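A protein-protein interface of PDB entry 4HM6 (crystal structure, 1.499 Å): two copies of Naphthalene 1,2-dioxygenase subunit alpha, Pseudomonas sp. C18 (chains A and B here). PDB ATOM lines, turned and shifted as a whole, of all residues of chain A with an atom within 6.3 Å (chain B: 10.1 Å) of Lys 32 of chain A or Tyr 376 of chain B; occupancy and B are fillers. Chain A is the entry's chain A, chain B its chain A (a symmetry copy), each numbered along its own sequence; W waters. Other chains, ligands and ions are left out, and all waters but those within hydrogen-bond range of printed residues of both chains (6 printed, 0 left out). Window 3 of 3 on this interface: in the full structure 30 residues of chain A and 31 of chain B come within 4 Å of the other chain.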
ATOM      1  N   PHE A  27      10.066  16.664  23.432  1.00  0.00           N
ATOM      2  CA  PHE A  27       8.926  16.098  22.726  1.00  0.00           C
ATOM      3  C   PHE A  27       7.663  16.876  23.103  1.00  0.00           C
ATOM      4  O   PHE A  27       6.891  17.284  22.238  1.00  0.00           O
ATOM      5  CB  PHE A  27       8.766  14.595  23.031  1.00  0.00           C
ATOM      6  CG  PHE A  27       7.572  13.965  22.357  1.00  0.00           C
ATOM      7  CD1 PHE A  27       6.319  14.013  22.959  1.00  0.00           C
ATOM      8  CD2 PHE A  27       7.700  13.326  21.127  1.00  0.00           C
ATOM      9  CE1 PHE A  27       5.199  13.448  22.345  1.00  0.00           C
ATOM     10  CE2 PHE A  27       6.597  12.752  20.500  1.00  0.00           C
ATOM     11  CZ  PHE A  27       5.341  12.806  21.110  1.00  0.00           C
ATOM     12  N   GLN A  28       7.449  17.084  24.394  1.00  0.00           N
ATOM     13  CA  GLN A  28       6.284  17.844  24.838  1.00  0.00           C
ATOM     14  C   GLN A  28       6.292  19.263  24.266  1.00  0.00           C
ATOM     15  O   GLN A  28       5.249  19.780  23.847  1.00  0.00           O
ATOM     16  CB  GLN A  28       6.203  17.865  26.368  1.00  0.00           C
ATOM     17  CG  GLN A  28       5.918  16.490  26.968  1.00  0.00           C
ATOM     18  CD  GLN A  28       4.549  15.962  26.582  1.00  0.00           C
ATOM     19  OE1 GLN A  28       3.552  16.689  26.653  1.00  0.00           O
ATOM     20  NE2 GLN A  28       4.489  14.691  26.172  1.00  0.00           N
ATOM     21  N   HIS A  29       7.472  19.874  24.207  1.00  0.00           N
ATOM     22  CA  HIS A  29       7.625  21.196  23.611  1.00  0.00           C
ATOM     23  C   HIS A  29       7.321  21.190  22.104  1.00  0.00           C
ATOM     24  O   HIS A  29       6.767  22.159  21.575  1.00  0.00           O
ATOM     25  CB  HIS A  29       9.033  21.738  23.894  1.00  0.00           C
ATOM     26  CG  HIS A  29       9.264  23.125  23.384  1.00  0.00           C
ATOM     27  ND1 HIS A  29       8.662  24.230  23.945  1.00  0.00           N
ATOM     28  CD2 HIS A  29      10.033  23.590  22.369  1.00  0.00           C
ATOM     29  CE1 HIS A  29       9.053  25.318  23.302  1.00  0.00           C
ATOM     30  NE2 HIS A  29       9.885  24.955  22.339  1.00  0.00           N
ATOM     31  N   GLU A  30       7.673  20.104  21.417  1.00  0.00           N
ATOM     32  CA  GLU A  30       7.374  19.957  19.993  1.00  0.00           C
ATOM     33  C   GLU A  30       5.868  19.872  19.743  1.00  0.00           C
ATOM     34  O   GLU A  30       5.391  20.278  18.687  1.00  0.00           O
ATOM     35  CB  GLU A  30       8.029  18.691  19.435  1.00  0.00           C
ATOM     36  CG  GLU A  30       9.516  18.748  19.262  1.00  0.00           C
ATOM     37  CD  GLU A  30      10.082  17.404  18.840  1.00  0.00           C
ATOM     38  OE1 GLU A  30       9.340  16.395  18.918  1.00  0.00           O
ATOM     39  OE2 GLU A  30      11.261  17.352  18.432  1.00  0.00           O
ATOM     40  N   LEU A  31       5.119  19.316  20.689  1.00  0.00           N
ATOM     41  CA  LEU A  31       3.665  19.261  20.535  1.00  0.00           C
ATOM     42  C   LEU A  31       3.129  20.670  20.320  1.00  0.00           C
ATOM     43  O   LEU A  31       2.276  20.896  19.460  1.00  0.00           O
ATOM     44  CB  LEU A  31       2.985  18.590  21.738  1.00  0.00           C
ATOM     45  CG  LEU A  31       3.370  17.140  22.005  1.00  0.00           C
ATOM     46  CD1 LEU A  31       2.599  16.599  23.200  1.00  0.00           C
ATOM     47  CD2 LEU A  31       3.119  16.289  20.763  1.00  0.00           C
ATOM     48  N   LYS A  32       3.675  21.623  21.072  1.00  0.00           N
ATOM     49  CA  LYS A  32       3.292  23.024  20.942  1.00  0.00           C
ATOM     50  C   LYS A  32       3.896  23.732  19.725  1.00  0.00           C
ATOM     51  O   LYS A  32       3.180  24.360  18.940  1.00  0.00           O
ATOM     52  CB  LYS A  32       3.693  23.775  22.212  1.00  0.00           C
ATOM     53  CG  LYS A  32       3.400  25.261  22.168  1.00  0.00           C
ATOM     54  CD  LYS A  32       3.574  25.892  23.533  1.00  0.00           C
ATOM     55  CE  LYS A  32       4.968  25.658  24.089  1.00  0.00           C
ATOM     56  NZ  LYS A  32       5.167  26.434  25.364  1.00  0.00           N
ATOM     57  N   THR A  33       5.212  23.644  19.569  1.00  0.00           N
ATOM     58  CA  THR A  33       5.919  24.488  18.593  1.00  0.00           C
ATOM     59  C   THR A  33       6.088  23.860  17.208  1.00  0.00           C
ATOM     60  O   THR A  33       6.401  24.560  16.234  1.00  0.00           O
ATOM     61  CB  THR A  33       7.299  24.935  19.114  1.00  0.00           C
ATOM     62  OG1 THR A  33       8.112  23.779  19.347  1.00  0.00           O
ATOM     63  CG2 THR A  33       7.155  25.736  20.412  1.00  0.00           C
ATOM     64  N   ILE A  34       5.893  22.547  17.117  1.00  0.00           N
ATOM     65  CA  ILE A  34       5.948  21.862  15.826  1.00  0.00           C
ATOM     66  C   ILE A  34       4.553  21.420  15.394  1.00  0.00           C
ATOM     67  O   ILE A  34       4.037  21.880  14.371  1.00  0.00           O
ATOM     68  CB  ILE A  34       6.889  20.633  15.837  1.00  0.00           C
ATOM     69  CG1 ILE A  34       8.329  21.044  16.178  1.00  0.00           C
ATOM     70  CG2 ILE A  34       6.826  19.909  14.485  1.00  0.00           C
ATOM     71  CD1 ILE A  34       9.000  21.962  15.147  1.00  0.00           C
ATOM     72  N   PHE A  35       3.932  20.545  16.179  1.00  0.00           N
ATOM     73  CA  PHE A  35       2.688  19.912  15.746  1.00  0.00           C
ATOM     74  C   PHE A  35       1.428  20.782  15.845  1.00  0.00           C
ATOM     75  O   PHE A  35       0.525  20.656  15.011  1.00  0.00           O
ATOM     76  CB  PHE A  35       2.510  18.547  16.435  1.00  0.00           C
ATOM     77  CG  PHE A  35       3.573  17.565  16.055  1.00  0.00           C
ATOM     78  CD1 PHE A  35       3.520  16.914  14.828  1.00  0.00           C
ATOM     79  CD2 PHE A  35       4.663  17.338  16.893  1.00  0.00           C
ATOM     80  CE1 PHE A  35       4.519  16.021  14.452  1.00  0.00           C
ATOM     81  CE2 PHE A  35       5.667  16.446  16.529  1.00  0.00           C
ATOM     82  CZ  PHE A  35       5.596  15.791  15.300  1.00  0.00           C
ATOM     83  N   ALA A  36       1.364  21.683  16.826  1.00  0.00           N
ATOM     84  CA  ALA A  36       0.192  22.556  16.936  1.00  0.00           C
ATOM     85  C   ALA A  36       0.318  23.772  16.023  1.00  0.00           C
ATOM     86  O   ALA A  36      -0.633  24.538  15.860  1.00  0.00           O
ATOM     87  CB  ALA A  36      -0.036  23.000  18.387  1.00  0.00           C
ATOM     88  N   ARG A  37       1.487  23.928  15.408  1.00  0.00           N
ATOM     89  CA  ARG A  37       1.784  25.124  14.629  1.00  0.00           C
ATOM     90  C   ARG A  37       1.805  24.896  13.118  1.00  0.00           C
ATOM     91  O   ARG A  37       1.483  25.801  12.340  1.00  0.00           O
ATOM     92  CB  ARG A  37       3.123  25.718  15.072  1.00  0.00           C
ATOM     93  CG  ARG A  37       3.418  27.050  14.375  1.00  0.00           C
ATOM     94  CD  ARG A  37       4.657  27.705  14.873  1.00  0.00           C
ATOM     95  NE  ARG A  37       4.627  27.917  16.311  1.00  0.00           N
ATOM     96  CZ  ARG A  37       5.721  28.048  17.045  1.00  0.00           C
ATOM     97  NH1 ARG A  37       6.908  27.991  16.451  1.00  0.00           N
ATOM     98  NH2 ARG A  37       5.630  28.224  18.355  1.00  0.00           N
ATOM     99  N   ILE A  61      -0.256  14.188  18.712  1.00  0.00           N
ATOM    100  CA  ILE A  61      -0.859  13.118  19.523  1.00  0.00           C
ATOM    101  C   ILE A  61      -2.382  13.237  19.614  1.00  0.00           C
ATOM    102  O   ILE A  61      -3.053  12.376  20.206  1.00  0.00           O
ATOM    103  CB  ILE A  61      -0.270  13.047  20.952  1.00  0.00           C
ATOM    104  CG1 ILE A  61      -0.571  14.328  21.739  1.00  0.00           C
ATOM    105  CG2 ILE A  61       1.237  12.761  20.908  1.00  0.00           C
ATOM    106  CD1 ILE A  61      -0.244  14.209  23.225  1.00  0.00           C
ATOM    107  N   ASP A  62      -2.933  14.303  19.042  1.00  0.00           N
ATOM    108  CA  ASP A  62      -4.383  14.474  19.023  1.00  0.00           C
ATOM    109  C   ASP A  62      -5.012  13.658  17.909  1.00  0.00           C
ATOM    110  O   ASP A  62      -4.361  13.371  16.900  1.00  0.00           O
ATOM    111  CB  ASP A  62      -4.743  15.950  18.863  1.00  0.00           C
ATOM    112  CG  ASP A  62      -4.245  16.790  20.015  1.00  0.00           C
ATOM    113  OD1 ASP A  62      -4.907  16.787  21.066  1.00  0.00           O
ATOM    114  OD2 ASP A  62      -3.191  17.443  19.882  1.00  0.00           O
ATOM    115  N   LYS A 136     -14.475  20.885  18.867  1.00  0.00           N
ATOM    116  CA  LYS A 136     -13.345  21.790  18.693  1.00  0.00           C
ATOM    117  C   LYS A 136     -12.785  21.615  17.288  1.00  0.00           C
ATOM    118  O   LYS A 136     -12.282  20.546  16.933  1.00  0.00           O
ATOM    119  CB  LYS A 136     -12.266  21.528  19.746  1.00  0.00           C
ATOM    120  CG  LYS A 136     -11.041  22.427  19.634  1.00  0.00           C
ATOM    121  CD  LYS A 136     -10.229  22.398  20.927  1.00  0.00           C
ATOM    122  CE  LYS A 136      -8.924  23.170  20.803  1.00  0.00           C
ATOM    123  NZ  LYS A 136      -8.217  23.254  22.111  1.00  0.00           N
ATOM    124  N   HIS B  18      -9.810  19.290  31.487  1.00  0.00           N
ATOM    125  CA  HIS B  18      -9.704  17.887  31.086  1.00  0.00           C
ATOM    126  C   HIS B  18      -8.378  17.292  31.554  1.00  0.00           C
ATOM    127  O   HIS B  18      -8.297  16.094  31.834  1.00  0.00           O
ATOM    128  CB  HIS B  18      -9.888  17.766  29.565  1.00  0.00           C
ATOM    129  CG  HIS B  18     -10.309  16.403  29.089  1.00  0.00           C
ATOM    130  ND1 HIS B  18     -10.841  16.194  27.838  1.00  0.00           N
ATOM    131  CD2 HIS B  18     -10.266  15.190  29.691  1.00  0.00           C
ATOM    132  CE1 HIS B  18     -11.116  14.907  27.686  1.00  0.00           C
ATOM    133  NE2 HIS B  18     -10.769  14.276  28.792  1.00  0.00           N
ATOM    134  N   LEU B  19      -7.348  18.132  31.686  1.00  0.00           N
ATOM    135  CA  LEU B  19      -6.042  17.667  32.158  1.00  0.00           C
ATOM    136  C   LEU B  19      -6.102  16.962  33.514  1.00  0.00           C
ATOM    137  O   LEU B  19      -5.216  16.172  33.836  1.00  0.00           O
ATOM    138  CB  LEU B  19      -5.021  18.817  32.204  1.00  0.00           C
ATOM    139  CG  LEU B  19      -5.215  19.857  33.316  1.00  0.00           C
ATOM    140  CD1 LEU B  19      -4.477  19.491  34.602  1.00  0.00           C
ATOM    141  CD2 LEU B  19      -4.773  21.229  32.840  1.00  0.00           C
ATOM    142  N   GLY B  22      -5.481  13.341  33.251  1.00  0.00           N
ATOM    143  CA  GLY B  22      -4.283  12.855  32.579  1.00  0.00           C
ATOM    144  C   GLY B  22      -2.944  13.331  33.127  1.00  0.00           C
ATOM    145  O   GLY B  22      -1.906  12.759  32.815  1.00  0.00           O
ATOM    146  N   SER B 370     -10.364   9.555  30.126  1.00  0.00           N
ATOM    147  CA  SER B 370      -9.162   9.773  30.917  1.00  0.00           C
ATOM    148  C   SER B 370      -7.958  10.007  30.028  1.00  0.00           C
ATOM    149  O   SER B 370      -7.173  10.916  30.267  1.00  0.00           O
ATOM    150  CB  SER B 370      -8.882   8.588  31.842  1.00  0.00           C
ATOM    151  OG  SER B 370      -9.962   8.355  32.720  1.00  0.00           O
ATOM    152  N   GLN B 371      -7.799   9.179  29.004  1.00  0.00           N
ATOM    153  CA  GLN B 371      -6.610   9.271  28.165  1.00  0.00           C
ATOM    154  C   GLN B 371      -6.607  10.543  27.306  1.00  0.00           C
ATOM    155  O   GLN B 371      -5.541  11.104  26.990  1.00  0.00           O
ATOM    156  CB  GLN B 371      -6.481   8.010  27.314  1.00  0.00           C
ATOM    157  CG  GLN B 371      -6.236   6.764  28.166  1.00  0.00           C
ATOM    158  CD  GLN B 371      -6.363   5.478  27.380  1.00  0.00           C
ATOM    159  OE1 GLN B 371      -6.166   5.468  26.166  1.00  0.00           O
ATOM    160  NE2 GLN B 371      -6.698   4.386  28.064  1.00  0.00           N
ATOM    161  N   ASN B 372      -7.793  11.018  26.951  1.00  0.00           N
ATOM    162  CA  ASN B 372      -7.890  12.261  26.197  1.00  0.00           C
ATOM    163  C   ASN B 372      -7.387  13.443  27.010  1.00  0.00           C
ATOM    164  O   ASN B 372      -6.992  14.458  26.446  1.00  0.00           O
ATOM    165  CB  ASN B 372      -9.330  12.504  25.714  1.00  0.00           C
ATOM    166  CG  ASN B 372      -9.704  11.615  24.550  1.00  0.00           C
ATOM    167  OD1 ASN B 372      -8.831  11.142  23.820  1.00  0.00           O
ATOM    168  ND2 ASN B 372     -10.998  11.376  24.370  1.00  0.00           N
ATOM    169  N   GLY B 373      -7.381  13.295  28.334  1.00  0.00           N
ATOM    170  CA  GLY B 373      -6.881  14.329  29.218  1.00  0.00           C
ATOM    171  C   GLY B 373      -5.392  14.575  29.080  1.00  0.00           C
ATOM    172  O   GLY B 373      -4.888  15.585  29.579  1.00  0.00           O
ATOM    173  N   LYS B 374      -4.693  13.663  28.402  1.00  0.00           N
ATOM    174  CA  LYS B 374      -3.268  13.839  28.125  1.00  0.00           C
ATOM    175  C   LYS B 374      -3.023  14.495  26.777  1.00  0.00           C
ATOM    176  O   LYS B 374      -1.924  14.990  26.520  1.00  0.00           O
ATOM    177  CB  LYS B 374      -2.532  12.495  28.146  1.00  0.00           C
ATOM    178  CG  LYS B 374      -2.419  11.845  29.513  1.00  0.00           C
ATOM    179  CD  LYS B 374      -1.600  10.550  29.429  1.00  0.00           C
ATOM    180  CE  LYS B 374      -1.269   9.970  30.809  1.00  0.00           C
ATOM    181  NZ  LYS B 374      -0.343  10.840  31.607  1.00  0.00           N
ATOM    182  N   LYS B 375      -4.031  14.485  25.909  1.00  0.00           N
ATOM    183  CA  LYS B 375      -3.855  14.965  24.541  1.00  0.00           C
ATOM    184  C   LYS B 375      -3.745  16.482  24.505  1.00  0.00           C
ATOM    185  O   LYS B 375      -4.501  17.185  25.175  1.00  0.00           O
ATOM    186  CB  LYS B 375      -4.978  14.447  23.629  1.00  0.00           C
ATOM    187  CG  LYS B 375      -4.901  12.941  23.405  1.00  0.00           C
ATOM    188  CD  LYS B 375      -5.931  12.467  22.399  1.00  0.00           C
ATOM    189  CE  LYS B 375      -5.765  10.982  22.090  1.00  0.00           C
ATOM    190  NZ  LYS B 375      -6.400  10.112  23.128  1.00  0.00           N
ATOM    191  N   TYR B 376      -2.788  16.966  23.722  1.00  0.00           N
ATOM    192  CA  TYR B 376      -2.397  18.374  23.746  1.00  0.00           C
ATOM    193  C   TYR B 376      -3.565  19.347  23.581  1.00  0.00           C
ATOM    194  O   TYR B 376      -3.676  20.329  24.336  1.00  0.00           O
ATOM    195  CB  TYR B 376      -1.325  18.652  22.678  1.00  0.00           C
ATOM    196  CG  TYR B 376      -0.845  20.085  22.714  1.00  0.00           C
ATOM    197  CD1 TYR B 376       0.158  20.480  23.594  1.00  0.00           C
ATOM    198  CD2 TYR B 376      -1.422  21.051  21.903  1.00  0.00           C
ATOM    199  CE1 TYR B 376       0.595  21.805  23.642  1.00  0.00           C
ATOM    200  CE2 TYR B 376      -1.005  22.369  21.948  1.00  0.00           C
ATOM    201  CZ  TYR B 376       0.003  22.746  22.819  1.00  0.00           C
ATOM    202  OH  TYR B 376       0.414  24.067  22.860  1.00  0.00           O
ATOM    203  N   GLN B 377      -4.425  19.103  22.593  1.00  0.00           N
ATOM    204  CA  GLN B 377      -5.509  20.049  22.320  1.00  0.00           C
ATOM    205  C   GLN B 377      -6.660  19.953  23.311  1.00  0.00           C
ATOM    206  O   GLN B 377      -7.593  20.773  23.275  1.00  0.00           O
ATOM    207  CB  GLN B 377      -6.038  19.884  20.890  1.00  0.00           C
ATOM    208  CG  GLN B 377      -5.047  20.277  19.800  1.00  0.00           C
ATOM    209  CD  GLN B 377      -4.759  21.775  19.765  1.00  0.00           C
ATOM    210  OE1 GLN B 377      -5.607  22.598  20.111  1.00  0.00           O
ATOM    211  NE2 GLN B 377      -3.548  22.130  19.353  1.00  0.00           N
ATOM    212  N   SER B 378      -6.607  18.959  24.196  1.00  0.00           N
ATOM    213  CA  SER B 378      -7.690  18.765  25.161  1.00  0.00           C
ATOM    214  C   SER B 378      -7.342  19.133  26.596  1.00  0.00           C
ATOM    215  O   SER B 378      -8.239  19.285  27.418  1.00  0.00           O
ATOM    216  CB  SER B 378      -8.213  17.327  25.126  1.00  0.00           C
ATOM    217  OG  SER B 378      -8.872  17.051  23.906  1.00  0.00           O
ATOM    218  N   ARG B 379      -6.053  19.251  26.905  1.00  0.00           N
ATOM    219  CA  ARG B 379      -5.624  19.485  28.281  1.00  0.00           C
ATOM    220  C   ARG B 379      -6.329  20.679  28.921  1.00  0.00           C
ATOM    221  O   ARG B 379      -6.788  20.592  30.062  1.00  0.00           O
ATOM    222  CB  ARG B 379      -4.104  19.687  28.337  1.00  0.00           C
ATOM    223  CG  ARG B 379      -3.276  18.421  28.071  1.00  0.00           C
ATOM    224  CD  ARG B 379      -1.815  18.768  27.817  1.00  0.00           C
ATOM    225  NE  ARG B 379      -1.092  17.646  27.227  1.00  0.00           N
ATOM    226  CZ  ARG B 379       0.178  17.686  26.815  1.00  0.00           C
ATOM    227  NH1 ARG B 379       0.907  18.799  26.926  1.00  0.00           N
ATOM    228  NH2 ARG B 379       0.723  16.599  26.285  1.00  0.00           N
ATOM    229  N   ASP B 380      -6.440  21.775  28.169  1.00  0.00           N
ATOM    230  CA  ASP B 380      -7.000  23.030  28.664  1.00  0.00           C
ATOM    231  C   ASP B 380      -8.484  23.160  28.307  1.00  0.00           C
ATOM    232  O   ASP B 380      -9.087  24.231  28.458  1.00  0.00           O
ATOM    233  CB  ASP B 380      -6.186  24.213  28.099  1.00  0.00           C
ATOM    234  CG  ASP B 380      -6.609  25.562  28.664  1.00  0.00           C
ATOM    235  OD1 ASP B 380      -6.755  25.674  29.902  1.00  0.00           O
ATOM    236  OD2 ASP B 380      -6.804  26.513  27.860  1.00  0.00           O
ATOM    237  N   SER B 381      -9.084  22.069  27.838  1.00  0.00           N
ATOM    238  CA  SER B 381     -10.513  22.090  27.521  1.00  0.00           C
ATOM    239  C   SER B 381     -11.355  21.859  28.767  1.00  0.00           C
ATOM    240  O   SER B 381     -10.853  21.374  29.781  1.00  0.00           O
ATOM    241  CB  SER B 381     -10.857  21.054  26.449  1.00  0.00           C
ATOM    242  OG  SER B 381     -10.206  21.364  25.227  1.00  0.00           O
HETATM  243  O   HOH W   1      -7.441  16.072  21.795  1.00  0.00           O
HETATM  244  O   HOH W   2       3.552  18.282  28.972  1.00  0.00           O
HETATM  245  O   HOH W   3      -7.865  23.184  25.031  1.00  0.00           O
HETATM  246  O   HOH W   4       1.757  13.448  26.021  1.00  0.00           O
HETATM  247  O   HOH W   5       3.199  20.045  25.726  1.00  0.00           O
HETATM  248  O   HOH W   6      -5.600  24.881  22.604  1.00  0.00           O
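Leu 31 of chain A touches Tyr 376 of chain B (CB to CD1, 3.9 Å).
Arg 379 of chain B touches Leu 31 of chain A (NH2 to CD1, 3.6 Å).
CG of Lys 32 of chain A touches OH of Tyr 376 of chain B, 3.3 Å away.
Ala 36 of chain A touches Tyr 376 of chain B (CB to CE2, 3.7 Å).
Ala 36 of chain A touches Gln 377 of chain B (CB to NE2, 3.7 Å).
Ile 61 of chain A touches Lys 374 of chain B (CD1 to O, 3.8 Å).
O of Ile 61 of chain A touches CE of Lys 375 of chain B, 3.6 Å away.
N of Tyr 376 of chain B touches CD1 of Ile 61 of chain A, 3.8 Å away.
Asp 62 of chain A touches Lys 375 of chain B.
Water W1 bridges OG of Ser 378 of chain B (2.7 Å) and OD1 of Asp 62 of chain A (2.7 Å).
Water W5 bridges the backbone carbonyl oxygen (O) of Gln 28 of chain A (2.8 Å) and the guanidinium group (NH1) of Arg 379 of chain B (2.9 Å).
Water W2 bridges the side-chain amide oxygen (OE1) of Gln 28 of chain A (2.8 Å) and the guanidinium group (NH1) of Arg 379 of chain B (3.4 Å).
Water W3 lies within hydrogen-bond range of the side-chain amino group (NZ) of Lys 136 of chain A (2.9 Å), the side-chain hydroxyl (OG) of Ser 381 of chain B (3.0 Å) and the backbone carbonyl oxygen (O) of Gln 377 of chain B (3.0 Å).
Water W4 bridges the side-chain amide nitrogen of Gln 28 of chain A (3.0 Å) and the guanidinium group of Arg 379 of chain B (3.3 Å).
Water W6 bridges NZ of Lys 136 of chain A (3.1 Å) and OE1 of Gln 377 of chain B (3.4 Å).
Of the 15 printed residues of chain B, 5 touch a printed residue of chain A.
Along chain B the printed residues that touch a printed residue of chain A span positions 374 to 379.
Printed residues of chain A that touch a printed residue of chain B: Gln 28, Leu 31, Lys 32, Ala 36, Ile 61, Asp 62 and Lys 136.
Lys 32 of chain A touches one residue of chain B.
No residue of chain B comes within 4 Å of Thr 33 of chain A.
Ala 36 of chain A touches just these residues of chain B: Tyr 376 (3.7 Å) and Gln 377 (3.7 Å).
Of the printed residues of chain B, Ile 61 of chain A touches Lys 374, Lys 375 and Tyr 376.
Of the printed residues of chain B, Lys 136 of chain A touches Gln 377.
Tyr 376 of chain B touches just these residues of chain A: Leu 31, Lys 32, Ala 36, Ile 61 and Asp 62.
Ser 378 of chain B touches none of the printed residues of chain A.
Printed residues of chain A within 4 Å of Arg 379 of chain B: Gln 28 and Leu 31.
The nearest printed residue of chain B that does not touch Lys 32 of chain A is Arg 379 of chain B (7.1 Å).
The nearest residue of chain A that does not touch Tyr 376 of chain B is Gln 28 of chain A (5.1 Å).
The nearest printed residue of chain A that does not touch Gln 377 of chain B is Leu 31 of chain A (6.0 Å).
No position is printed for both chains.
O of Leu 31 of chain A lies within hydrogen-bond range of N of Ala 36 of chain A, 2.9 Å away.
N of Leu 19 of chain B is in hydrogen-bond range of O of Arg 379 of chain B (3.0 Å).
The side-chain amino group of Lys 374 of chain B is in hydrogen-bond range of the backbone carbonyl oxygen of Gly 22 of chain B (2.8 Å).
The side-chain amide oxygen (OD1) of Asn 372 of chain B sits at hydrogen-bond distance from the side-chain amino group (NZ) of Lys 375 of chain B (2.7 Å).
O of Lys 374 of chain B sits at hydrogen-bond distance from NE of Arg 379 of chain B.
O of Gln 377 of chain B sits at hydrogen-bond distance from OG of Ser 381 of chain B (3.3 Å).
The guanidinium group (NH2) of Arg 379 of chain B is in hydrogen-bond range of the side-chain amide oxygen (OE1) of Gln 28 of chain A, at 2.9 Å.
N of Tyr 376 of chain B lies within hydrogen-bond range of OD1 of Asp 62 of chain A (3.4 Å).
OD1 of Asp 62 of chain A sits at hydrogen-bond distance from N of Gln 377 of chain B (2.8 Å).
The side-chain amino group (NZ) of Lys 136 of chain A is in hydrogen-bond range of the backbone carbonyl oxygen (O) of Gln 377 of chain B, 2.8 Å away.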
